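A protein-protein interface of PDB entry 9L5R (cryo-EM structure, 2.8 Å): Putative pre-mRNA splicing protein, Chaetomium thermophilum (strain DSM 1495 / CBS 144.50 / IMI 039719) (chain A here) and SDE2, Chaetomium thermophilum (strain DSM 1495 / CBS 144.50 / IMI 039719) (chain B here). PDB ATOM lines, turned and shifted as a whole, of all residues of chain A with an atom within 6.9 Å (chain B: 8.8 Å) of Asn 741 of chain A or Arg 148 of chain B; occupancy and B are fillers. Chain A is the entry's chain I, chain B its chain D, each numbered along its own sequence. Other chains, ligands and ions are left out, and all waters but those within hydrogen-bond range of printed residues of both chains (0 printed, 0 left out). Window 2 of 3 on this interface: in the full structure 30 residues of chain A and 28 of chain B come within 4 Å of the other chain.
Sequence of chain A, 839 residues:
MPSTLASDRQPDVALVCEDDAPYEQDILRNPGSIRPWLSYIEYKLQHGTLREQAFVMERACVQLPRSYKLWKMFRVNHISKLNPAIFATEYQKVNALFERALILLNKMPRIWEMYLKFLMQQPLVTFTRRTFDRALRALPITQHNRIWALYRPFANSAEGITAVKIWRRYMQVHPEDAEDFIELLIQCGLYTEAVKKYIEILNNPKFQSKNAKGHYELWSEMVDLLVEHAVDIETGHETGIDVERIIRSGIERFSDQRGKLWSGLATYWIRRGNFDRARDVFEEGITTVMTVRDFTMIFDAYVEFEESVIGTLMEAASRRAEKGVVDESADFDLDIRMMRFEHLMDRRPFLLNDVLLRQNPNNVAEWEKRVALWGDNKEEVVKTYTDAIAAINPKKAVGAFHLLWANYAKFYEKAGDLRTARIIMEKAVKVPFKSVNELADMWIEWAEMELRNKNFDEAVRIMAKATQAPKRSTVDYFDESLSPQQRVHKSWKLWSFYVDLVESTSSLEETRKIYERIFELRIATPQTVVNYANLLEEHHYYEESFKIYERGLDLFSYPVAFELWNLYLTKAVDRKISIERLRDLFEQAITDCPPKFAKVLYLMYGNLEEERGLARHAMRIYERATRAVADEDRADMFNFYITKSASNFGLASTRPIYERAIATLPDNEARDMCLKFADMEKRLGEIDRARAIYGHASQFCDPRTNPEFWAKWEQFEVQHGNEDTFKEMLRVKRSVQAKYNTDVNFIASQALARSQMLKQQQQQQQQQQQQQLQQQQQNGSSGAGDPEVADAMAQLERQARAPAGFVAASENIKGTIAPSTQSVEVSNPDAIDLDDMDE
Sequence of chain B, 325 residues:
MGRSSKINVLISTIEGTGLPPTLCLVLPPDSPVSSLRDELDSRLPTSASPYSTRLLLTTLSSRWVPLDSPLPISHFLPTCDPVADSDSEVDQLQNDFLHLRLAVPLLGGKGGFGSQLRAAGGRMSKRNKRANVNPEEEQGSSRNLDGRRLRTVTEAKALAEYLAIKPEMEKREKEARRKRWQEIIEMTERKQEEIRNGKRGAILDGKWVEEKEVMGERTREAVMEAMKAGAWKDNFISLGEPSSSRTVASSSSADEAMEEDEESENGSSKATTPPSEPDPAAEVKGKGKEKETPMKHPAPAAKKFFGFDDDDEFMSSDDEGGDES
Of the 16 printed residues of chain A, 4 touch a printed residue of chain B. Of the 17 printed residues of chain B, 5 touch a printed residue of chain A. Hydrophobic or aromatic side chains of chain B that line the printed part of chain A: Ala 156. Among the printed residues, no Asp or Glu carboxylate lies within 4 Å of a Lys or Arg side-chain nitrogen of the other chain.
Of chain B, only Arg 148 (2.3 Å) comes within 4 Å of Asn 741 of chain A. Of chain A, only Asn 741 (2.3 Å), Asp 743 (3.3 Å) and Phe 746 (3.2 Å) come within 4 Å of Arg 148 of chain B. No residue of chain B comes within 4 Å of Thr 742 of chain A. No residue of chain A comes within 4 Å of Gly 147 of chain B. Printed residues of chain A within 4 Å of Thr 152 of chain B: Asp 743 (3.6 Å), Phe 746 (3.7 Å) and Ile 747 (3.2 Å). Of the printed residues of chain B, Asp 743 of chain A touches Arg 148 (3.3 Å), Arg 149 (3.9 Å) and Thr 152 (3.6 Å). Asn 745 of chain A touches none of the printed residues of chain B. Thr 154 of chain B touches none of the printed residues of chain A.
The backbone carbonyl oxygen of Phe 746 of chain A lies within hydrogen-bond range of the side-chain hydroxyl of Ser 749 of chain A. O of Ser 141 of chain B is in hydrogen-bond range of NH1 of Arg 149 of chain B, 2.7 Å away. The side-chain hydroxyl (OG1) of Thr 152 of chain B is in hydrogen-bond range of the backbone carbonyl oxygen (O) of Arg 149 of chain B, 2.4 Å away.
Among the printed residues, pairs that only touch across the chains: Asp 743 of chain A with Arg 148 of chain B (3.3 Å), Asp 743 of chain A with Arg 149 of chain B (3.9 Å), Asp 743 of chain A with Thr 152 of chain B (3.6 Å), Phe 746 of chain A with Arg 148 of chain B (3.2 Å), Phe 746 of chain A with Thr 152 of chain B (3.7 Å), Phe 746 of chain A with Val 153 of chain B (3.99 Å), Phe 746 of chain A with Ala 156 of chain B (3.6 Å), Ile 747 of chain A with Thr 152 of chain B (3.2 Å) and Ile 747 of chain A with Ala 156 of chain B (3.4 Å).
OD1 of Asn 741 of chain A lies close to NH2 of Arg 148 of chain B.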
ATOM      1  N   ASP A 702      13.767   0.179  11.448  1.00  0.00           N
ATOM      2  CA  ASP A 702      13.849   0.356  12.896  1.00  0.00           C
ATOM      3  C   ASP A 702      13.542   1.806  13.259  1.00  0.00           C
ATOM      4  O   ASP A 702      14.106   2.717  12.647  1.00  0.00           O
ATOM      5  CB  ASP A 702      15.244  -0.046  13.372  1.00  0.00           C
ATOM      6  CG  ASP A 702      15.518   0.322  14.814  1.00  0.00           C
ATOM      7  OD1 ASP A 702      14.617   0.211  15.663  1.00  0.00           O
ATOM      8  OD2 ASP A 702      16.672   0.684  15.105  1.00  0.00           O
ATOM      9  N   ARG A 704      14.278   3.908  15.760  1.00  0.00           N
ATOM     10  CA  ARG A 704      15.296   4.830  16.241  1.00  0.00           C
ATOM     11  C   ARG A 704      16.365   5.120  15.199  1.00  0.00           C
ATOM     12  O   ARG A 704      17.300   5.872  15.490  1.00  0.00           O
ATOM     13  CB  ARG A 704      15.938   4.308  17.527  1.00  0.00           C
ATOM     14  CG  ARG A 704      16.654   2.992  17.392  1.00  0.00           C
ATOM     15  CD  ARG A 704      16.817   2.325  18.743  1.00  0.00           C
ATOM     16  NE  ARG A 704      17.306   0.958  18.622  1.00  0.00           N
ATOM     17  CZ  ARG A 704      17.436   0.119  19.639  1.00  0.00           C
ATOM     18  NH1 ARG A 704      17.127   0.476  20.873  1.00  0.00           N
ATOM     19  NH2 ARG A 704      17.888  -1.110  19.412  1.00  0.00           N
ATOM     20  N   SER A 735       5.896  -3.077  18.127  1.00  0.00           N
ATOM     21  CA  SER A 735       6.353  -4.436  17.855  1.00  0.00           C
ATOM     22  C   SER A 735       7.712  -4.433  17.165  1.00  0.00           C
ATOM     23  O   SER A 735       8.572  -5.266  17.474  1.00  0.00           O
ATOM     24  CB  SER A 735       5.325  -5.178  17.007  1.00  0.00           C
ATOM     25  OG  SER A 735       5.474  -4.859  15.640  1.00  0.00           O
ATOM     26  N   VAL A 736       7.924  -3.503  16.232  1.00  0.00           N
ATOM     27  CA  VAL A 736       9.217  -3.388  15.564  1.00  0.00           C
ATOM     28  C   VAL A 736      10.283  -2.913  16.546  1.00  0.00           C
ATOM     29  O   VAL A 736      11.439  -3.352  16.491  1.00  0.00           O
ATOM     30  CB  VAL A 736       9.095  -2.468  14.337  1.00  0.00           C
ATOM     31  CG1 VAL A 736      10.440  -2.193  13.723  1.00  0.00           C
ATOM     32  CG2 VAL A 736       8.208  -3.110  13.302  1.00  0.00           C
ATOM     33  N   GLN A 737       9.907  -2.034  17.476  1.00  0.00           N
ATOM     34  CA  GLN A 737      10.828  -1.644  18.542  1.00  0.00           C
ATOM     35  C   GLN A 737      11.230  -2.840  19.397  1.00  0.00           C
ATOM     36  O   GLN A 737      12.405  -2.990  19.758  1.00  0.00           O
ATOM     37  CB  GLN A 737      10.194  -0.566  19.417  1.00  0.00           C
ATOM     38  CG  GLN A 737      10.088   0.779  18.757  1.00  0.00           C
ATOM     39  CD  GLN A 737       9.363   1.781  19.616  1.00  0.00           C
ATOM     40  OE1 GLN A 737       9.311   2.967  19.295  1.00  0.00           O
ATOM     41  NE2 GLN A 737       8.790   1.312  20.714  1.00  0.00           N
ATOM     42  N   ALA A 738      10.266  -3.702  19.726  1.00  0.00           N
ATOM     43  CA  ALA A 738      10.572  -4.916  20.479  1.00  0.00           C
ATOM     44  C   ALA A 738      11.485  -5.850  19.694  1.00  0.00           C
ATOM     45  O   ALA A 738      12.394  -6.461  20.265  1.00  0.00           O
ATOM     46  CB  ALA A 738       9.279  -5.631  20.862  1.00  0.00           C
ATOM     47  N   LYS A 739      11.243  -5.986  18.386  1.00  0.00           N
ATOM     48  CA  LYS A 739      12.089  -6.837  17.553  1.00  0.00           C
ATOM     49  C   LYS A 739      13.521  -6.320  17.505  1.00  0.00           C
ATOM     50  O   LYS A 739      14.478  -7.093  17.631  1.00  0.00           O
ATOM     51  CB  LYS A 739      11.520  -6.925  16.140  1.00  0.00           C
ATOM     52  CG  LYS A 739      12.550  -7.309  15.097  1.00  0.00           C
ATOM     53  CD  LYS A 739      12.006  -7.247  13.694  1.00  0.00           C
ATOM     54  CE  LYS A 739      13.094  -7.564  12.689  1.00  0.00           C
ATOM     55  NZ  LYS A 739      12.556  -7.697  11.311  1.00  0.00           N
ATOM     56  N   TYR A 740      13.690  -5.014  17.353  1.00  0.00           N
ATOM     57  CA  TYR A 740      15.010  -4.419  17.264  1.00  0.00           C
ATOM     58  C   TYR A 740      15.599  -4.096  18.628  1.00  0.00           C
ATOM     59  O   TYR A 740      16.655  -3.464  18.699  1.00  0.00           O
ATOM     60  CB  TYR A 740      14.955  -3.165  16.397  1.00  0.00           C
ATOM     61  CG  TYR A 740      14.935  -3.463  14.920  1.00  0.00           C
ATOM     62  CD1 TYR A 740      13.745  -3.678  14.257  1.00  0.00           C
ATOM     63  CD2 TYR A 740      16.110  -3.536  14.193  1.00  0.00           C
ATOM     64  CE1 TYR A 740      13.721  -3.955  12.913  1.00  0.00           C
ATOM     65  CE2 TYR A 740      16.098  -3.813  12.847  1.00  0.00           C
ATOM     66  CZ  TYR A 740      14.900  -4.021  12.213  1.00  0.00           C
ATOM     67  OH  TYR A 740      14.887  -4.294  10.867  1.00  0.00           O
ATOM     68  N   ASN A 741      14.950  -4.521  19.710  1.00  0.00           N
ATOM     69  CA  ASN A 741      15.434  -4.275  21.069  1.00  0.00           C
ATOM     70  C   ASN A 741      16.579  -5.221  21.449  1.00  0.00           C
ATOM     71  O   ASN A 741      16.533  -5.924  22.456  1.00  0.00           O
ATOM     72  CB  ASN A 741      14.275  -4.423  22.045  1.00  0.00           C
ATOM     73  CG  ASN A 741      14.510  -3.705  23.348  1.00  0.00           C
ATOM     74  OD1 ASN A 741      15.116  -2.638  23.379  1.00  0.00           O
ATOM     75  ND2 ASN A 741      14.057  -4.303  24.442  1.00  0.00           N
ATOM     76  N   THR A 742      17.636  -5.225  20.639  1.00  0.00           N
ATOM     77  CA  THR A 742      18.781  -6.094  20.879  1.00  0.00           C
ATOM     78  C   THR A 742      20.045  -5.271  21.089  1.00  0.00           C
ATOM     79  O   THR A 742      20.092  -4.070  20.814  1.00  0.00           O
ATOM     80  CB  THR A 742      19.003  -7.086  19.728  1.00  0.00           C
ATOM     81  OG1 THR A 742      19.440  -6.384  18.560  1.00  0.00           O
ATOM     82  CG2 THR A 742      17.734  -7.861  19.423  1.00  0.00           C
ATOM     83  N   ASP A 743      21.079  -5.957  21.584  1.00  0.00           N
ATOM     84  CA  ASP A 743      22.361  -5.313  21.853  1.00  0.00           C
ATOM     85  C   ASP A 743      23.020  -4.812  20.576  1.00  0.00           C
ATOM     86  O   ASP A 743      23.613  -3.730  20.563  1.00  0.00           O
ATOM     87  CB  ASP A 743      23.291  -6.280  22.579  1.00  0.00           C
ATOM     88  CG  ASP A 743      22.848  -6.558  24.000  1.00  0.00           C
ATOM     89  OD1 ASP A 743      22.217  -5.670  24.607  1.00  0.00           O
ATOM     90  OD2 ASP A 743      23.138  -7.658  24.514  1.00  0.00           O
ATOM     91  N   VAL A 744      22.933  -5.592  19.499  1.00  0.00           N
ATOM     92  CA  VAL A 744      23.538  -5.218  18.222  1.00  0.00           C
ATOM     93  C   VAL A 744      22.909  -3.940  17.675  1.00  0.00           C
ATOM     94  O   VAL A 744      23.604  -2.992  17.272  1.00  0.00           O
ATOM     95  CB  VAL A 744      23.393  -6.384  17.231  1.00  0.00           C
ATOM     96  CG1 VAL A 744      23.848  -5.985  15.869  1.00  0.00           C
ATOM     97  CG2 VAL A 744      24.185  -7.569  17.726  1.00  0.00           C
ATOM     98  N   ASN A 745      21.579  -3.895  17.667  1.00  0.00           N
ATOM     99  CA  ASN A 745      20.884  -2.707  17.203  1.00  0.00           C
ATOM    100  C   ASN A 745      21.097  -1.537  18.149  1.00  0.00           C
ATOM    101  O   ASN A 745      21.088  -0.385  17.710  1.00  0.00           O
ATOM    102  CB  ASN A 745      19.404  -3.018  17.038  1.00  0.00           C
ATOM    103  CG  ASN A 745      19.151  -4.007  15.934  1.00  0.00           C
ATOM    104  OD1 ASN A 745      19.772  -3.939  14.876  1.00  0.00           O
ATOM    105  ND2 ASN A 745      18.255  -4.952  16.179  1.00  0.00           N
ATOM    106  N   PHE A 746      21.314  -1.812  19.437  1.00  0.00           N
ATOM    107  CA  PHE A 746      21.666  -0.749  20.373  1.00  0.00           C
ATOM    108  C   PHE A 746      23.016  -0.136  20.028  1.00  0.00           C
ATOM    109  O   PHE A 746      23.169   1.088  20.071  1.00  0.00           O
ATOM    110  CB  PHE A 746      21.677  -1.296  21.795  1.00  0.00           C
ATOM    111  CG  PHE A 746      22.249  -0.352  22.816  1.00  0.00           C
ATOM    112  CD1 PHE A 746      21.488   0.684  23.318  1.00  0.00           C
ATOM    113  CD2 PHE A 746      23.533  -0.522  23.298  1.00  0.00           C
ATOM    114  CE1 PHE A 746      21.995   1.533  24.271  1.00  0.00           C
ATOM    115  CE2 PHE A 746      24.049   0.337  24.244  1.00  0.00           C
ATOM    116  CZ  PHE A 746      23.280   1.365  24.728  1.00  0.00           C
ATOM    117  N   ILE A 747      24.004  -0.975  19.698  1.00  0.00           N
ATOM    118  CA  ILE A 747      25.315  -0.475  19.280  1.00  0.00           C
ATOM    119  C   ILE A 747      25.172   0.411  18.051  1.00  0.00           C
ATOM    120  O   ILE A 747      25.685   1.538  18.010  1.00  0.00           O
ATOM    121  CB  ILE A 747      26.284  -1.635  18.990  1.00  0.00           C
ATOM    122  CG1 ILE A 747      26.485  -2.544  20.201  1.00  0.00           C
ATOM    123  CG2 ILE A 747      27.619  -1.089  18.504  1.00  0.00           C
ATOM    124  CD1 ILE A 747      27.474  -2.061  21.183  1.00  0.00           C
ATOM    125  N   SER A 749      22.482   1.970  16.841  1.00  0.00           N
ATOM    126  CA  SER A 749      21.691   3.173  17.067  1.00  0.00           C
ATOM    127  C   SER A 749      22.450   4.202  17.895  1.00  0.00           C
ATOM    128  O   SER A 749      22.361   5.401  17.619  1.00  0.00           O
ATOM    129  CB  SER A 749      20.374   2.813  17.746  1.00  0.00           C
ATOM    130  OG  SER A 749      20.604   2.240  19.018  1.00  0.00           O
ATOM    131  N   GLN B 139      32.673  -7.320  35.086  1.00  0.00           N
ATOM    132  CA  GLN B 139      31.308  -7.817  34.969  1.00  0.00           C
ATOM    133  C   GLN B 139      30.668  -7.411  33.647  1.00  0.00           C
ATOM    134  O   GLN B 139      29.478  -7.111  33.585  1.00  0.00           O
ATOM    135  CB  GLN B 139      30.464  -7.341  36.144  1.00  0.00           C
ATOM    136  CG  GLN B 139      30.660  -8.179  37.391  1.00  0.00           C
ATOM    137  CD  GLN B 139      29.429  -8.228  38.271  1.00  0.00           C
ATOM    138  OE1 GLN B 139      28.608  -9.141  38.165  1.00  0.00           O
ATOM    139  NE2 GLN B 139      29.298  -7.250  39.160  1.00  0.00           N
ATOM    140  N   GLY B 140      31.467  -7.409  32.575  1.00  0.00           N
ATOM    141  CA  GLY B 140      30.991  -6.964  31.276  1.00  0.00           C
ATOM    142  C   GLY B 140      29.865  -7.790  30.685  1.00  0.00           C
ATOM    143  O   GLY B 140      29.090  -7.289  29.871  1.00  0.00           O
ATOM    144  N   SER B 141      29.752  -9.052  31.073  1.00  0.00           N
ATOM    145  CA  SER B 141      28.677  -9.889  30.562  1.00  0.00           C
ATOM    146  C   SER B 141      27.422  -9.837  31.416  1.00  0.00           C
ATOM    147  O   SER B 141      26.427 -10.470  31.062  1.00  0.00           O
ATOM    148  CB  SER B 141      29.147 -11.332  30.424  1.00  0.00           C
ATOM    149  OG  SER B 141      30.144 -11.437  29.427  1.00  0.00           O
ATOM    150  N   SER B 142      27.439  -9.095  32.518  1.00  0.00           N
ATOM    151  CA  SER B 142      26.256  -8.915  33.340  1.00  0.00           C
ATOM    152  C   SER B 142      25.326  -7.895  32.692  1.00  0.00           C
ATOM    153  O   SER B 142      25.627  -7.323  31.647  1.00  0.00           O
ATOM    154  CB  SER B 142      26.657  -8.496  34.744  1.00  0.00           C
ATOM    155  OG  SER B 142      27.069  -9.613  35.500  1.00  0.00           O
ATOM    156  N   ARG B 143      24.187  -7.640  33.319  1.00  0.00           N
ATOM    157  CA  ARG B 143      23.160  -6.819  32.699  1.00  0.00           C
ATOM    158  C   ARG B 143      22.823  -5.598  33.549  1.00  0.00           C
ATOM    159  O   ARG B 143      23.033  -5.577  34.763  1.00  0.00           O
ATOM    160  CB  ARG B 143      21.893  -7.635  32.446  1.00  0.00           C
ATOM    161  CG  ARG B 143      21.961  -8.473  31.204  1.00  0.00           C
ATOM    162  CD  ARG B 143      20.616  -9.065  30.888  1.00  0.00           C
ATOM    163  NE  ARG B 143      20.670  -9.897  29.695  1.00  0.00           N
ATOM    164  CZ  ARG B 143      20.908 -11.200  29.701  1.00  0.00           C
ATOM    165  NH1 ARG B 143      21.118 -11.859  30.825  1.00  0.00           N
ATOM    166  NH2 ARG B 143      20.935 -11.856  28.548  1.00  0.00           N
ATOM    167  N   ASN B 144      22.293  -4.577  32.876  1.00  0.00           N
ATOM    168  CA  ASN B 144      21.754  -3.382  33.514  1.00  0.00           C
ATOM    169  C   ASN B 144      20.350  -3.669  34.035  1.00  0.00           C
ATOM    170  O   ASN B 144      19.893  -4.813  34.066  1.00  0.00           O
ATOM    171  CB  ASN B 144      21.724  -2.216  32.532  1.00  0.00           C
ATOM    172  CG  ASN B 144      23.014  -1.446  32.491  1.00  0.00           C
ATOM    173  OD1 ASN B 144      23.642  -1.328  31.444  1.00  0.00           O
ATOM    174  ND2 ASN B 144      23.415  -0.903  33.633  1.00  0.00           N
ATOM    175  N   LEU B 145      19.637  -2.621  34.445  1.00  0.00           N
ATOM    176  CA  LEU B 145      18.231  -2.787  34.790  1.00  0.00           C
ATOM    177  C   LEU B 145      17.356  -2.897  33.554  1.00  0.00           C
ATOM    178  O   LEU B 145      16.291  -3.516  33.606  1.00  0.00           O
ATOM    179  CB  LEU B 145      17.722  -1.629  35.643  1.00  0.00           C
ATOM    180  CG  LEU B 145      17.949  -1.609  37.153  1.00  0.00           C
ATOM    181  CD1 LEU B 145      17.229  -2.773  37.819  1.00  0.00           C
ATOM    182  CD2 LEU B 145      19.405  -1.561  37.518  1.00  0.00           C
ATOM    183  N   ASP B 146      17.772  -2.291  32.444  1.00  0.00           N
ATOM    184  CA  ASP B 146      17.040  -2.399  31.190  1.00  0.00           C
ATOM    185  C   ASP B 146      17.534  -3.548  30.319  1.00  0.00           C
ATOM    186  O   ASP B 146      17.386  -3.502  29.091  1.00  0.00           O
ATOM    187  CB  ASP B 146      17.071  -1.061  30.444  1.00  0.00           C
ATOM    188  CG  ASP B 146      18.475  -0.596  30.098  1.00  0.00           C
ATOM    189  OD1 ASP B 146      19.455  -1.263  30.473  1.00  0.00           O
ATOM    190  OD2 ASP B 146      18.596   0.464  29.450  1.00  0.00           O
ATOM    191  N   GLY B 147      18.120  -4.575  30.932  1.00  0.00           N
ATOM    192  CA  GLY B 147      18.419  -5.814  30.247  1.00  0.00           C
ATOM    193  C   GLY B 147      19.532  -5.741  29.235  1.00  0.00           C
ATOM    194  O   GLY B 147      19.570  -6.559  28.316  1.00  0.00           O
ATOM    195  N   ARG B 148      20.441  -4.790  29.372  1.00  0.00           N
ATOM    196  CA  ARG B 148      21.495  -4.579  28.395  1.00  0.00           C
ATOM    197  C   ARG B 148      22.840  -4.899  29.020  1.00  0.00           C
ATOM    198  O   ARG B 148      23.088  -4.569  30.181  1.00  0.00           O
ATOM    199  CB  ARG B 148      21.459  -3.144  27.881  1.00  0.00           C
ATOM    200  CG  ARG B 148      20.137  -2.861  27.221  1.00  0.00           C
ATOM    201  CD  ARG B 148      20.021  -3.652  25.942  1.00  0.00           C
ATOM    202  NE  ARG B 148      18.747  -3.438  25.274  1.00  0.00           N
ATOM    203  CZ  ARG B 148      18.530  -2.486  24.383  1.00  0.00           C
ATOM    204  NH1 ARG B 148      19.423  -1.548  24.153  1.00  0.00           N
ATOM    205  NH2 ARG B 148      17.379  -2.463  23.723  1.00  0.00           N
ATOM    206  N   ARG B 149      23.699  -5.558  28.251  1.00  0.00           N
ATOM    207  CA  ARG B 149      24.991  -5.958  28.778  1.00  0.00           C
ATOM    208  C   ARG B 149      25.919  -4.761  28.911  1.00  0.00           C
ATOM    209  O   ARG B 149      25.948  -3.860  28.062  1.00  0.00           O
ATOM    210  CB  ARG B 149      25.624  -7.030  27.896  1.00  0.00           C
ATOM    211  CG  ARG B 149      24.873  -8.348  27.904  1.00  0.00           C
ATOM    212  CD  ARG B 149      25.789  -9.516  27.631  1.00  0.00           C
ATOM    213  NE  ARG B 149      25.044 -10.678  27.164  1.00  0.00           N
ATOM    214  CZ  ARG B 149      24.790 -11.755  27.895  1.00  0.00           C
ATOM    215  NH1 ARG B 149      25.215 -11.861  29.139  1.00  0.00           N
ATOM    216  NH2 ARG B 149      24.098 -12.752  27.359  1.00  0.00           N
ATOM    217  N   LEU B 150      26.676  -4.756  30.012  1.00  0.00           N
ATOM    218  CA  LEU B 150      27.586  -3.655  30.297  1.00  0.00           C
ATOM    219  C   LEU B 150      28.672  -3.546  29.241  1.00  0.00           C
ATOM    220  O   LEU B 150      29.118  -2.438  28.914  1.00  0.00           O
ATOM    221  CB  LEU B 150      28.208  -3.835  31.681  1.00  0.00           C
ATOM    222  CG  LEU B 150      27.274  -4.166  32.845  1.00  0.00           C
ATOM    223  CD1 LEU B 150      28.039  -4.134  34.144  1.00  0.00           C
ATOM    224  CD2 LEU B 150      26.111  -3.209  32.908  1.00  0.00           C
ATOM    225  N   ARG B 151      29.092  -4.681  28.679  1.00  0.00           N
ATOM    226  CA  ARG B 151      30.035  -4.632  27.576  1.00  0.00           C
ATOM    227  C   ARG B 151      29.405  -4.016  26.338  1.00  0.00           C
ATOM    228  O   ARG B 151      30.099  -3.352  25.572  1.00  0.00           O
ATOM    229  CB  ARG B 151      30.591  -6.029  27.278  1.00  0.00           C
ATOM    230  CG  ARG B 151      29.639  -6.983  26.587  1.00  0.00           C
ATOM    231  CD  ARG B 151      30.334  -8.241  26.112  1.00  0.00           C
ATOM    232  NE  ARG B 151      29.371  -9.175  25.543  1.00  0.00           N
ATOM    233  CZ  ARG B 151      29.083  -9.262  24.253  1.00  0.00           C
ATOM    234  NH1 ARG B 151      29.712  -8.527  23.352  1.00  0.00           N
ATOM    235  NH2 ARG B 151      28.138 -10.106  23.857  1.00  0.00           N
ATOM    236  N   THR B 152      28.093  -4.166  26.147  1.00  0.00           N
ATOM    237  CA  THR B 152      27.468  -3.516  25.004  1.00  0.00           C
ATOM    238  C   THR B 152      27.323  -2.023  25.224  1.00  0.00           C
ATOM    239  O   THR B 152      27.444  -1.253  24.270  1.00  0.00           O
ATOM    240  CB  THR B 152      26.107  -4.126  24.706  1.00  0.00           C
ATOM    241  OG1 THR B 152      25.204  -3.820  25.771  1.00  0.00           O
ATOM    242  CG2 THR B 152      26.240  -5.619  24.573  1.00  0.00           C
ATOM    243  N   VAL B 153      27.089  -1.596  26.463  1.00  0.00           N
ATOM    244  CA  VAL B 153      27.109  -0.165  26.762  1.00  0.00           C
ATOM    245  C   VAL B 153      28.489   0.416  26.462  1.00  0.00           C
ATOM    246  O   VAL B 153      28.621   1.450  25.785  1.00  0.00           O
ATOM    247  CB  VAL B 153      26.688   0.079  28.221  1.00  0.00           C
ATOM    248  CG1 VAL B 153      27.176   1.428  28.706  1.00  0.00           C
ATOM    249  CG2 VAL B 153      25.183  -0.019  28.351  1.00  0.00           C
ATOM    250  N   THR B 154      29.536  -0.276  26.917  1.00  0.00           N
ATOM    251  CA  THR B 154      30.901   0.191  26.700  1.00  0.00           C
ATOM    252  C   THR B 154      31.262   0.218  25.218  1.00  0.00           C
ATOM    253  O   THR B 154      31.848   1.194  24.733  1.00  0.00           O
ATOM    254  CB  THR B 154      31.871  -0.692  27.485  1.00  0.00           C
ATOM    255  OG1 THR B 154      31.628  -0.529  28.886  1.00  0.00           O
ATOM    256  CG2 THR B 154      33.312  -0.329  27.188  1.00  0.00           C
ATOM    257  N   ALA B 156      29.171   0.426  22.668  1.00  0.00           N
ATOM    258  CA  ALA B 156      28.407   1.471  21.994  1.00  0.00           C
ATOM    259  C   ALA B 156      29.052   2.831  22.194  1.00  0.00           C
ATOM    260  O   ALA B 156      29.155   3.623  21.249  1.00  0.00           O
ATOM    261  CB  ALA B 156      26.969   1.486  22.500  1.00  0.00           C
